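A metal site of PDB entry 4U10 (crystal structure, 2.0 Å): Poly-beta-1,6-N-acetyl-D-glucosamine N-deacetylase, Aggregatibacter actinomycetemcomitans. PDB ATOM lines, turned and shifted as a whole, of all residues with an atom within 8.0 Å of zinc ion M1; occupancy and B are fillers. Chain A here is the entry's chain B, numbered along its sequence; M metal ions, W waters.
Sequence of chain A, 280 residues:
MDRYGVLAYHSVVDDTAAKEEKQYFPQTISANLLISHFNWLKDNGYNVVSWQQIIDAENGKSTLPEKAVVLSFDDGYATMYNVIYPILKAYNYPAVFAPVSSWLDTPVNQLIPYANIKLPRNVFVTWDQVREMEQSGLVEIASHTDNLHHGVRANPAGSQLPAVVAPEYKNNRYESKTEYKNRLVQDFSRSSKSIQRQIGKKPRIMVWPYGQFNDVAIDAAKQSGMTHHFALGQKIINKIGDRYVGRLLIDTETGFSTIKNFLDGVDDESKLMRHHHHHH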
ATOM      1  N   TYR A   9      19.670 -10.624  -7.435  1.00  0.00           N
ATOM      2  CA  TYR A   9      18.332 -10.402  -8.036  1.00  0.00           C
ATOM      3  C   TYR A   9      17.407  -9.732  -7.005  1.00  0.00           C
ATOM      4  O   TYR A   9      17.683  -9.782  -5.779  1.00  0.00           O
ATOM      5  CB  TYR A   9      17.672 -11.704  -8.448  1.00  0.00           C
ATOM      6  CG  TYR A   9      18.341 -12.456  -9.584  1.00  0.00           C
ATOM      7  CD1 TYR A   9      18.024 -12.173 -10.910  1.00  0.00           C
ATOM      8  CD2 TYR A   9      19.267 -13.465  -9.334  1.00  0.00           C
ATOM      9  CE1 TYR A   9      18.614 -12.860 -11.940  1.00  0.00           C
ATOM     10  CE2 TYR A   9      19.878 -14.174 -10.373  1.00  0.00           C
ATOM     11  CZ  TYR A   9      19.555 -13.866 -11.662  1.00  0.00           C
ATOM     12  OH  TYR A   9      20.120 -14.553 -12.729  1.00  0.00           O
ATOM     13  N   HIS A  10      16.367  -9.062  -7.515  1.00  0.00           N
ATOM     14  CA  HIS A  10      15.373  -8.435  -6.669  1.00  0.00           C
ATOM     15  C   HIS A  10      14.012  -9.011  -7.043  1.00  0.00           C
ATOM     16  O   HIS A  10      13.848 -10.257  -6.924  1.00  0.00           O
ATOM     17  CB  HIS A  10      15.509  -6.906  -6.799  1.00  0.00           C
ATOM     18  CG  HIS A  10      16.751  -6.403  -6.145  1.00  0.00           C
ATOM     19  ND1 HIS A  10      17.985  -6.490  -6.764  1.00  0.00           N
ATOM     20  CD2 HIS A  10      16.995  -5.968  -4.900  1.00  0.00           C
ATOM     21  CE1 HIS A  10      18.910  -6.039  -5.961  1.00  0.00           C
ATOM     22  NE2 HIS A  10      18.343  -5.717  -4.815  1.00  0.00           N
ATOM     23  N   PRO A  26      13.158  -1.222  -7.984  1.00  0.00           N
ATOM     24  CA  PRO A  26      14.471  -1.183  -8.665  1.00  0.00           C
ATOM     25  C   PRO A  26      14.974  -2.576  -9.103  1.00  0.00           C
ATOM     26  O   PRO A  26      14.904  -3.463  -8.326  1.00  0.00           O
ATOM     27  CB  PRO A  26      15.398  -0.577  -7.567  1.00  0.00           C
ATOM     28  CG  PRO A  26      14.530   0.067  -6.574  1.00  0.00           C
ATOM     29  CD  PRO A  26      13.203  -0.726  -6.592  1.00  0.00           C
ATOM     30  N   PHE A  73      18.517 -13.226  -3.638  1.00  0.00           N
ATOM     31  CA  PHE A  73      17.306 -12.491  -3.976  1.00  0.00           C
ATOM     32  C   PHE A  73      17.039 -11.559  -2.749  1.00  0.00           C
ATOM     33  O   PHE A  73      17.014 -12.014  -1.618  1.00  0.00           O
ATOM     34  CB  PHE A  73      16.095 -13.451  -4.258  1.00  0.00           C
ATOM     35  CG  PHE A  73      16.321 -14.353  -5.441  1.00  0.00           C
ATOM     36  CD1 PHE A  73      16.998 -15.562  -5.292  1.00  0.00           C
ATOM     37  CD2 PHE A  73      15.911 -13.978  -6.710  1.00  0.00           C
ATOM     38  CE1 PHE A  73      17.218 -16.372  -6.364  1.00  0.00           C
ATOM     39  CE2 PHE A  73      16.208 -14.726  -7.810  1.00  0.00           C
ATOM     40  CZ  PHE A  73      16.867 -15.939  -7.644  1.00  0.00           C
ATOM     41  N   ASP A  74      16.957 -10.256  -3.010  1.00  0.00           N
ATOM     42  CA  ASP A  74      16.765  -9.302  -1.993  1.00  0.00           C
ATOM     43  C   ASP A  74      15.327  -8.770  -1.906  1.00  0.00           C
ATOM     44  O   ASP A  74      14.664  -8.508  -2.966  1.00  0.00           O
ATOM     45  CB  ASP A  74      17.642  -8.087  -2.222  1.00  0.00           C
ATOM     46  CG  ASP A  74      19.159  -8.355  -2.060  1.00  0.00           C
ATOM     47  OD1 ASP A  74      19.652  -9.486  -1.816  1.00  0.00           O
ATOM     48  OD2 ASP A  74      19.900  -7.369  -2.245  1.00  0.00           O
ATOM     49  N   ASP A  75      14.907  -8.581  -0.654  1.00  0.00           N
ATOM     50  CA  ASP A  75      13.876  -7.616  -0.204  1.00  0.00           C
ATOM     51  C   ASP A  75      12.654  -8.193   0.503  1.00  0.00           C
ATOM     52  O   ASP A  75      12.166  -7.606   1.477  1.00  0.00           O
ATOM     53  CB  ASP A  75      13.432  -6.610  -1.317  1.00  0.00           C
ATOM     54  CG  ASP A  75      14.517  -5.635  -1.700  1.00  0.00           C
ATOM     55  OD1 ASP A  75      15.561  -5.646  -1.054  1.00  0.00           O
ATOM     56  OD2 ASP A  75      14.325  -4.807  -2.653  1.00  0.00           O
ATOM     57  N   GLY A  76      12.228  -9.368   0.035  1.00  0.00           N
ATOM     58  CA  GLY A  76      11.066 -10.085   0.546  1.00  0.00           C
ATOM     59  C   GLY A  76       9.794 -10.027  -0.287  1.00  0.00           C
ATOM     60  O   GLY A  76       8.729 -10.308   0.218  1.00  0.00           O
ATOM     61  N   TYR A  77       9.907  -9.659  -1.551  1.00  0.00           N
ATOM     62  CA  TYR A  77       8.772  -9.545  -2.436  1.00  0.00           C
ATOM     63  C   TYR A  77       8.089 -10.884  -2.636  1.00  0.00           C
ATOM     64  O   TYR A  77       8.791 -11.927  -2.742  1.00  0.00           O
ATOM     65  CB  TYR A  77       9.168  -9.022  -3.811  1.00  0.00           C
ATOM     66  CG  TYR A  77       9.860  -7.708  -3.800  1.00  0.00           C
ATOM     67  CD1 TYR A  77       9.279  -6.581  -3.243  1.00  0.00           C
ATOM     68  CD2 TYR A  77      11.116  -7.590  -4.341  1.00  0.00           C
ATOM     69  CE1 TYR A  77       9.954  -5.354  -3.264  1.00  0.00           C
ATOM     70  CE2 TYR A  77      11.781  -6.408  -4.409  1.00  0.00           C
ATOM     71  CZ  TYR A  77      11.219  -5.292  -3.897  1.00  0.00           C
ATOM     72  OH  TYR A  77      11.982  -4.146  -3.934  1.00  0.00           O
ATOM     73  N   ALA A  98      16.961 -12.672   1.242  1.00  0.00           N
ATOM     74  CA  ALA A  98      17.154 -11.674   2.227  1.00  0.00           C
ATOM     75  C   ALA A  98      15.964 -10.741   2.294  1.00  0.00           C
ATOM     76  O   ALA A  98      15.981  -9.676   1.687  1.00  0.00           O
ATOM     77  CB  ALA A  98      18.453 -10.891   1.973  1.00  0.00           C
ATOM     78  N   PRO A  99      14.941 -11.137   3.043  1.00  0.00           N
ATOM     79  CA  PRO A  99      13.848 -10.204   3.336  1.00  0.00           C
ATOM     80  C   PRO A  99      14.115  -9.191   4.437  1.00  0.00           C
ATOM     81  O   PRO A  99      14.803  -9.471   5.422  1.00  0.00           O
ATOM     82  CB  PRO A  99      12.726 -11.146   3.750  1.00  0.00           C
ATOM     83  CG  PRO A  99      13.426 -12.274   4.505  1.00  0.00           C
ATOM     84  CD  PRO A  99      14.788 -12.412   3.807  1.00  0.00           C
ATOM     85  N   VAL A 100      13.548  -7.974   4.290  1.00  0.00           N
ATOM     86  CA  VAL A 100      13.467  -7.040   5.362  1.00  0.00           C
ATOM     87  C   VAL A 100      12.484  -7.519   6.411  1.00  0.00           C
ATOM     88  O   VAL A 100      11.273  -7.702   6.140  1.00  0.00           O
ATOM     89  CB  VAL A 100      13.061  -5.652   4.838  1.00  0.00           C
ATOM     90  CG1 VAL A 100      13.103  -4.614   5.954  1.00  0.00           C
ATOM     91  CG2 VAL A 100      14.016  -5.225   3.727  1.00  0.00           C
ATOM     92  N   TRP A 103       9.189  -5.639   7.543  1.00  0.00           N
ATOM     93  CA  TRP A 103       8.249  -5.594   6.438  1.00  0.00           C
ATOM     94  C   TRP A 103       7.456  -6.853   6.531  1.00  0.00           C
ATOM     95  O   TRP A 103       6.223  -6.800   6.588  1.00  0.00           O
ATOM     96  CB  TRP A 103       8.937  -5.471   5.104  1.00  0.00           C
ATOM     97  CG  TRP A 103       9.597  -4.157   4.885  1.00  0.00           C
ATOM     98  CD1 TRP A 103       9.607  -3.086   5.749  1.00  0.00           C
ATOM     99  CD2 TRP A 103      10.351  -3.755   3.756  1.00  0.00           C
ATOM    100  NE1 TRP A 103      10.303  -2.087   5.203  1.00  0.00           N
ATOM    101  CE2 TRP A 103      10.753  -2.461   3.963  1.00  0.00           C
ATOM    102  CE3 TRP A 103      10.678  -4.360   2.525  1.00  0.00           C
ATOM    103  CZ2 TRP A 103      11.483  -1.765   3.034  1.00  0.00           C
ATOM    104  CZ3 TRP A 103      11.387  -3.704   1.646  1.00  0.00           C
ATOM    105  CH2 TRP A 103      11.797  -2.414   1.885  1.00  0.00           C
ATOM    106  N   TYR A 114       7.352   3.143   3.028  1.00  0.00           N
ATOM    107  CA  TYR A 114       8.313   2.960   1.967  1.00  0.00           C
ATOM    108  C   TYR A 114       8.618   4.348   1.334  1.00  0.00           C
ATOM    109  O   TYR A 114       7.908   4.843   0.456  1.00  0.00           O
ATOM    110  CB  TYR A 114       7.728   2.003   0.979  1.00  0.00           C
ATOM    111  CG  TYR A 114       8.651   1.488  -0.082  1.00  0.00           C
ATOM    112  CD1 TYR A 114       9.525   0.462   0.187  1.00  0.00           C
ATOM    113  CD2 TYR A 114       8.604   1.976  -1.368  1.00  0.00           C
ATOM    114  CE1 TYR A 114      10.359  -0.064  -0.795  1.00  0.00           C
ATOM    115  CE2 TYR A 114       9.452   1.482  -2.374  1.00  0.00           C
ATOM    116  CZ  TYR A 114      10.319   0.450  -2.048  1.00  0.00           C
ATOM    117  OH  TYR A 114      11.152  -0.093  -2.958  1.00  0.00           O
ATOM    118  N   HIS A 144      18.426  -8.613   5.853  1.00  0.00           N
ATOM    119  CA  HIS A 144      18.470  -7.426   5.047  1.00  0.00           C
ATOM    120  C   HIS A 144      18.116  -6.218   5.868  1.00  0.00           C
ATOM    121  O   HIS A 144      17.626  -5.234   5.325  1.00  0.00           O
ATOM    122  CB  HIS A 144      17.499  -7.579   3.864  1.00  0.00           C
ATOM    123  CG  HIS A 144      17.852  -6.819   2.627  1.00  0.00           C
ATOM    124  ND1 HIS A 144      19.135  -6.617   2.181  1.00  0.00           N
ATOM    125  CD2 HIS A 144      17.038  -6.296   1.668  1.00  0.00           C
ATOM    126  CE1 HIS A 144      19.098  -5.953   1.029  1.00  0.00           C
ATOM    127  NE2 HIS A 144      17.826  -5.785   0.689  1.00  0.00           N
ATOM    128  N   THR A 145      18.507  -6.234   7.151  1.00  0.00           N
ATOM    129  CA  THR A 145      18.192  -5.335   8.217  1.00  0.00           C
ATOM    130  C   THR A 145      16.748  -5.451   8.630  1.00  0.00           C
ATOM    131  O   THR A 145      15.925  -6.043   7.903  1.00  0.00           O
ATOM    132  CB  THR A 145      18.506  -3.833   7.890  1.00  0.00           C
ATOM    133  OG1 THR A 145      17.471  -3.293   7.065  1.00  0.00           O
ATOM    134  CG2 THR A 145      19.877  -3.688   7.236  1.00  0.00           C
ATOM    135  N   HIS A 149      16.162  -0.220   5.650  1.00  0.00           N
ATOM    136  CA  HIS A 149      16.109  -0.220   4.202  1.00  0.00           C
ATOM    137  C   HIS A 149      15.433   1.008   3.645  1.00  0.00           C
ATOM    138  O   HIS A 149      14.449   0.914   2.868  1.00  0.00           O
ATOM    139  CB  HIS A 149      15.338  -1.393   3.677  1.00  0.00           C
ATOM    140  CG  HIS A 149      15.710  -1.819   2.300  1.00  0.00           C
ATOM    141  ND1 HIS A 149      15.358  -1.114   1.157  1.00  0.00           N
ATOM    142  CD2 HIS A 149      16.274  -2.978   1.866  1.00  0.00           C
ATOM    143  CE1 HIS A 149      15.784  -1.798   0.090  1.00  0.00           C
ATOM    144  NE2 HIS A 149      16.371  -2.918   0.502  1.00  0.00           N
ATOM    145  N   VAL A 207      22.978  -9.072   4.179  1.00  0.00           N
ATOM    146  CA  VAL A 207      22.984  -8.504   2.863  1.00  0.00           C
ATOM    147  C   VAL A 207      22.651  -7.022   2.971  1.00  0.00           C
ATOM    148  O   VAL A 207      21.533  -6.639   3.431  1.00  0.00           O
ATOM    149  CB  VAL A 207      21.910  -9.172   1.974  1.00  0.00           C
ATOM    150  CG1 VAL A 207      21.945  -8.585   0.581  1.00  0.00           C
ATOM    151  CG2 VAL A 207      22.013 -10.713   1.953  1.00  0.00           C
ATOM    152  N   TRP A 208      23.547  -6.157   2.454  1.00  0.00           N
ATOM    153  CA  TRP A 208      23.343  -4.706   2.573  1.00  0.00           C
ATOM    154  C   TRP A 208      22.342  -4.145   1.604  1.00  0.00           C
ATOM    155  O   TRP A 208      22.401  -4.427   0.406  1.00  0.00           O
ATOM    156  CB  TRP A 208      24.656  -3.952   2.391  1.00  0.00           C
ATOM    157  CG  TRP A 208      25.803  -4.480   3.228  1.00  0.00           C
ATOM    158  CD1 TRP A 208      26.932  -5.056   2.765  1.00  0.00           C
ATOM    159  CD2 TRP A 208      25.943  -4.407   4.630  1.00  0.00           C
ATOM    160  NE1 TRP A 208      27.758  -5.371   3.792  1.00  0.00           N
ATOM    161  CE2 TRP A 208      27.157  -5.011   4.956  1.00  0.00           C
ATOM    162  CE3 TRP A 208      25.117  -3.964   5.679  1.00  0.00           C
ATOM    163  CZ2 TRP A 208      27.602  -5.120   6.279  1.00  0.00           C
ATOM    164  CZ3 TRP A 208      25.570  -4.064   6.954  1.00  0.00           C
ATOM    165  CH2 TRP A 208      26.782  -4.640   7.250  1.00  0.00           C
ATOM    166  N   PRO A 209      21.333  -3.388   2.118  1.00  0.00           N
ATOM    167  CA  PRO A 209      20.432  -2.654   1.207  1.00  0.00           C
ATOM    168  C   PRO A 209      21.278  -1.832   0.273  1.00  0.00           C
ATOM    169  O   PRO A 209      22.254  -1.203   0.701  1.00  0.00           O
ATOM    170  CB  PRO A 209      19.631  -1.754   2.153  1.00  0.00           C
ATOM    171  CG  PRO A 209      19.699  -2.406   3.478  1.00  0.00           C
ATOM    172  CD  PRO A 209      20.921  -3.296   3.518  1.00  0.00           C
ATOM    173  N   TYR A 210      20.927  -1.892  -1.039  1.00  0.00           N
ATOM    174  CA  TYR A 210      21.541  -1.106  -2.110  1.00  0.00           C
ATOM    175  C   TYR A 210      23.005  -1.355  -2.255  1.00  0.00           C
ATOM    176  O   TYR A 210      23.657  -0.557  -2.907  1.00  0.00           O
ATOM    177  CB  TYR A 210      21.385   0.421  -1.909  1.00  0.00           C
ATOM    178  CG  TYR A 210      20.099   0.843  -1.215  1.00  0.00           C
ATOM    179  CD1 TYR A 210      18.864   0.730  -1.839  1.00  0.00           C
ATOM    180  CD2 TYR A 210      20.129   1.302   0.085  1.00  0.00           C
ATOM    181  CE1 TYR A 210      17.680   1.085  -1.192  1.00  0.00           C
ATOM    182  CE2 TYR A 210      18.960   1.660   0.760  1.00  0.00           C
ATOM    183  CZ  TYR A 210      17.736   1.560   0.097  1.00  0.00           C
ATOM    184  OH  TYR A 210      16.615   1.932   0.821  1.00  0.00           O
ATOM    185  N   GLY A 211      23.532  -2.400  -1.614  1.00  0.00           N
ATOM    186  CA  GLY A 211      24.976  -2.687  -1.731  1.00  0.00           C
ATOM    187  C   GLY A 211      25.836  -1.729  -0.919  1.00  0.00           C
ATOM    188  O   GLY A 211      27.075  -1.777  -1.011  1.00  0.00           O
ATOM    189  N   ARG A 247      28.839  -9.199  -5.379  1.00  0.00           N
ATOM    190  CA  ARG A 247      27.779  -9.770  -6.195  1.00  0.00           C
ATOM    191  C   ARG A 247      27.541  -9.008  -7.473  1.00  0.00           C
ATOM    192  O   ARG A 247      27.744  -7.807  -7.510  1.00  0.00           O
ATOM    193  CB  ARG A 247      26.436  -9.765  -5.426  1.00  0.00           C
ATOM    194  CG  ARG A 247      26.461 -10.340  -3.996  1.00  0.00           C
ATOM    195  CD  ARG A 247      25.021 -10.460  -3.399  1.00  0.00           C
ATOM    196  NE  ARG A 247      24.388  -9.152  -3.138  1.00  0.00           N
ATOM    197  CZ  ARG A 247      23.076  -8.982  -2.852  1.00  0.00           C
ATOM    198  NH1 ARG A 247      22.223 -10.034  -2.857  1.00  0.00           N
ATOM    199  NH2 ARG A 247      22.609  -7.775  -2.653  1.00  0.00           N
HETATM  200 ZN    ZN M   1      17.078  -4.434  -0.746  1.00  0.00          ZN
HETATM  201 ZN    ZN M   2      19.396  -5.460  -3.048  1.00  0.00          ZN
HETATM  202  O   HOH W   1      15.819  -2.572  -3.221  1.00  0.00           O
HETATM  203  O   HOH W   2      18.535  -4.283  -2.018  1.00  0.00           O
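Merely in contact with zinc ion M1: Asp 74. Four residues have an atom within 4 Å of zinc ion M1: Asp 74, Asp 75, His 144 and His 149.
The side-chain hydroxyl (OH) of Tyr 77 is in hydrogen-bond range of the side-chain carboxylate (OD2) of Asp 75 (2.8 Å). The backbone carbonyl oxygen (O) of Asp 75 is in hydrogen-bond range of the backbone NH (N) of Val 100, 3.2 Å away. OD1 of Asp 74 is in salt-bridge range of NH1 of Arg 247 (2.8 Å). The backbone NH (N) of Asp 75 is in hydrogen-bond range of the backbone carbonyl oxygen (O) of Ala 98, at 2.8 Å. The backbone NH (N) of Asp 74 is in hydrogen-bond range of the backbone carbonyl oxygen (O) of Tyr 9 (2.9 Å). O of His 149 lies within hydrogen-bond range of OH of Tyr 210 (3.1 Å). O of Val 207 is in hydrogen-bond range of ND1 of His 144.
Water W2 binds zinc ion M1, at 1.9 Å. The side-chain carboxylate (OD1) of Asp 75 binds zinc ion M1 (2.0 Å). NE2 of His 149 is bound to zinc ion M1, 2.1 Å away. Zinc ion M1 is bound by NE2 of His 144, at 2.1 Å.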
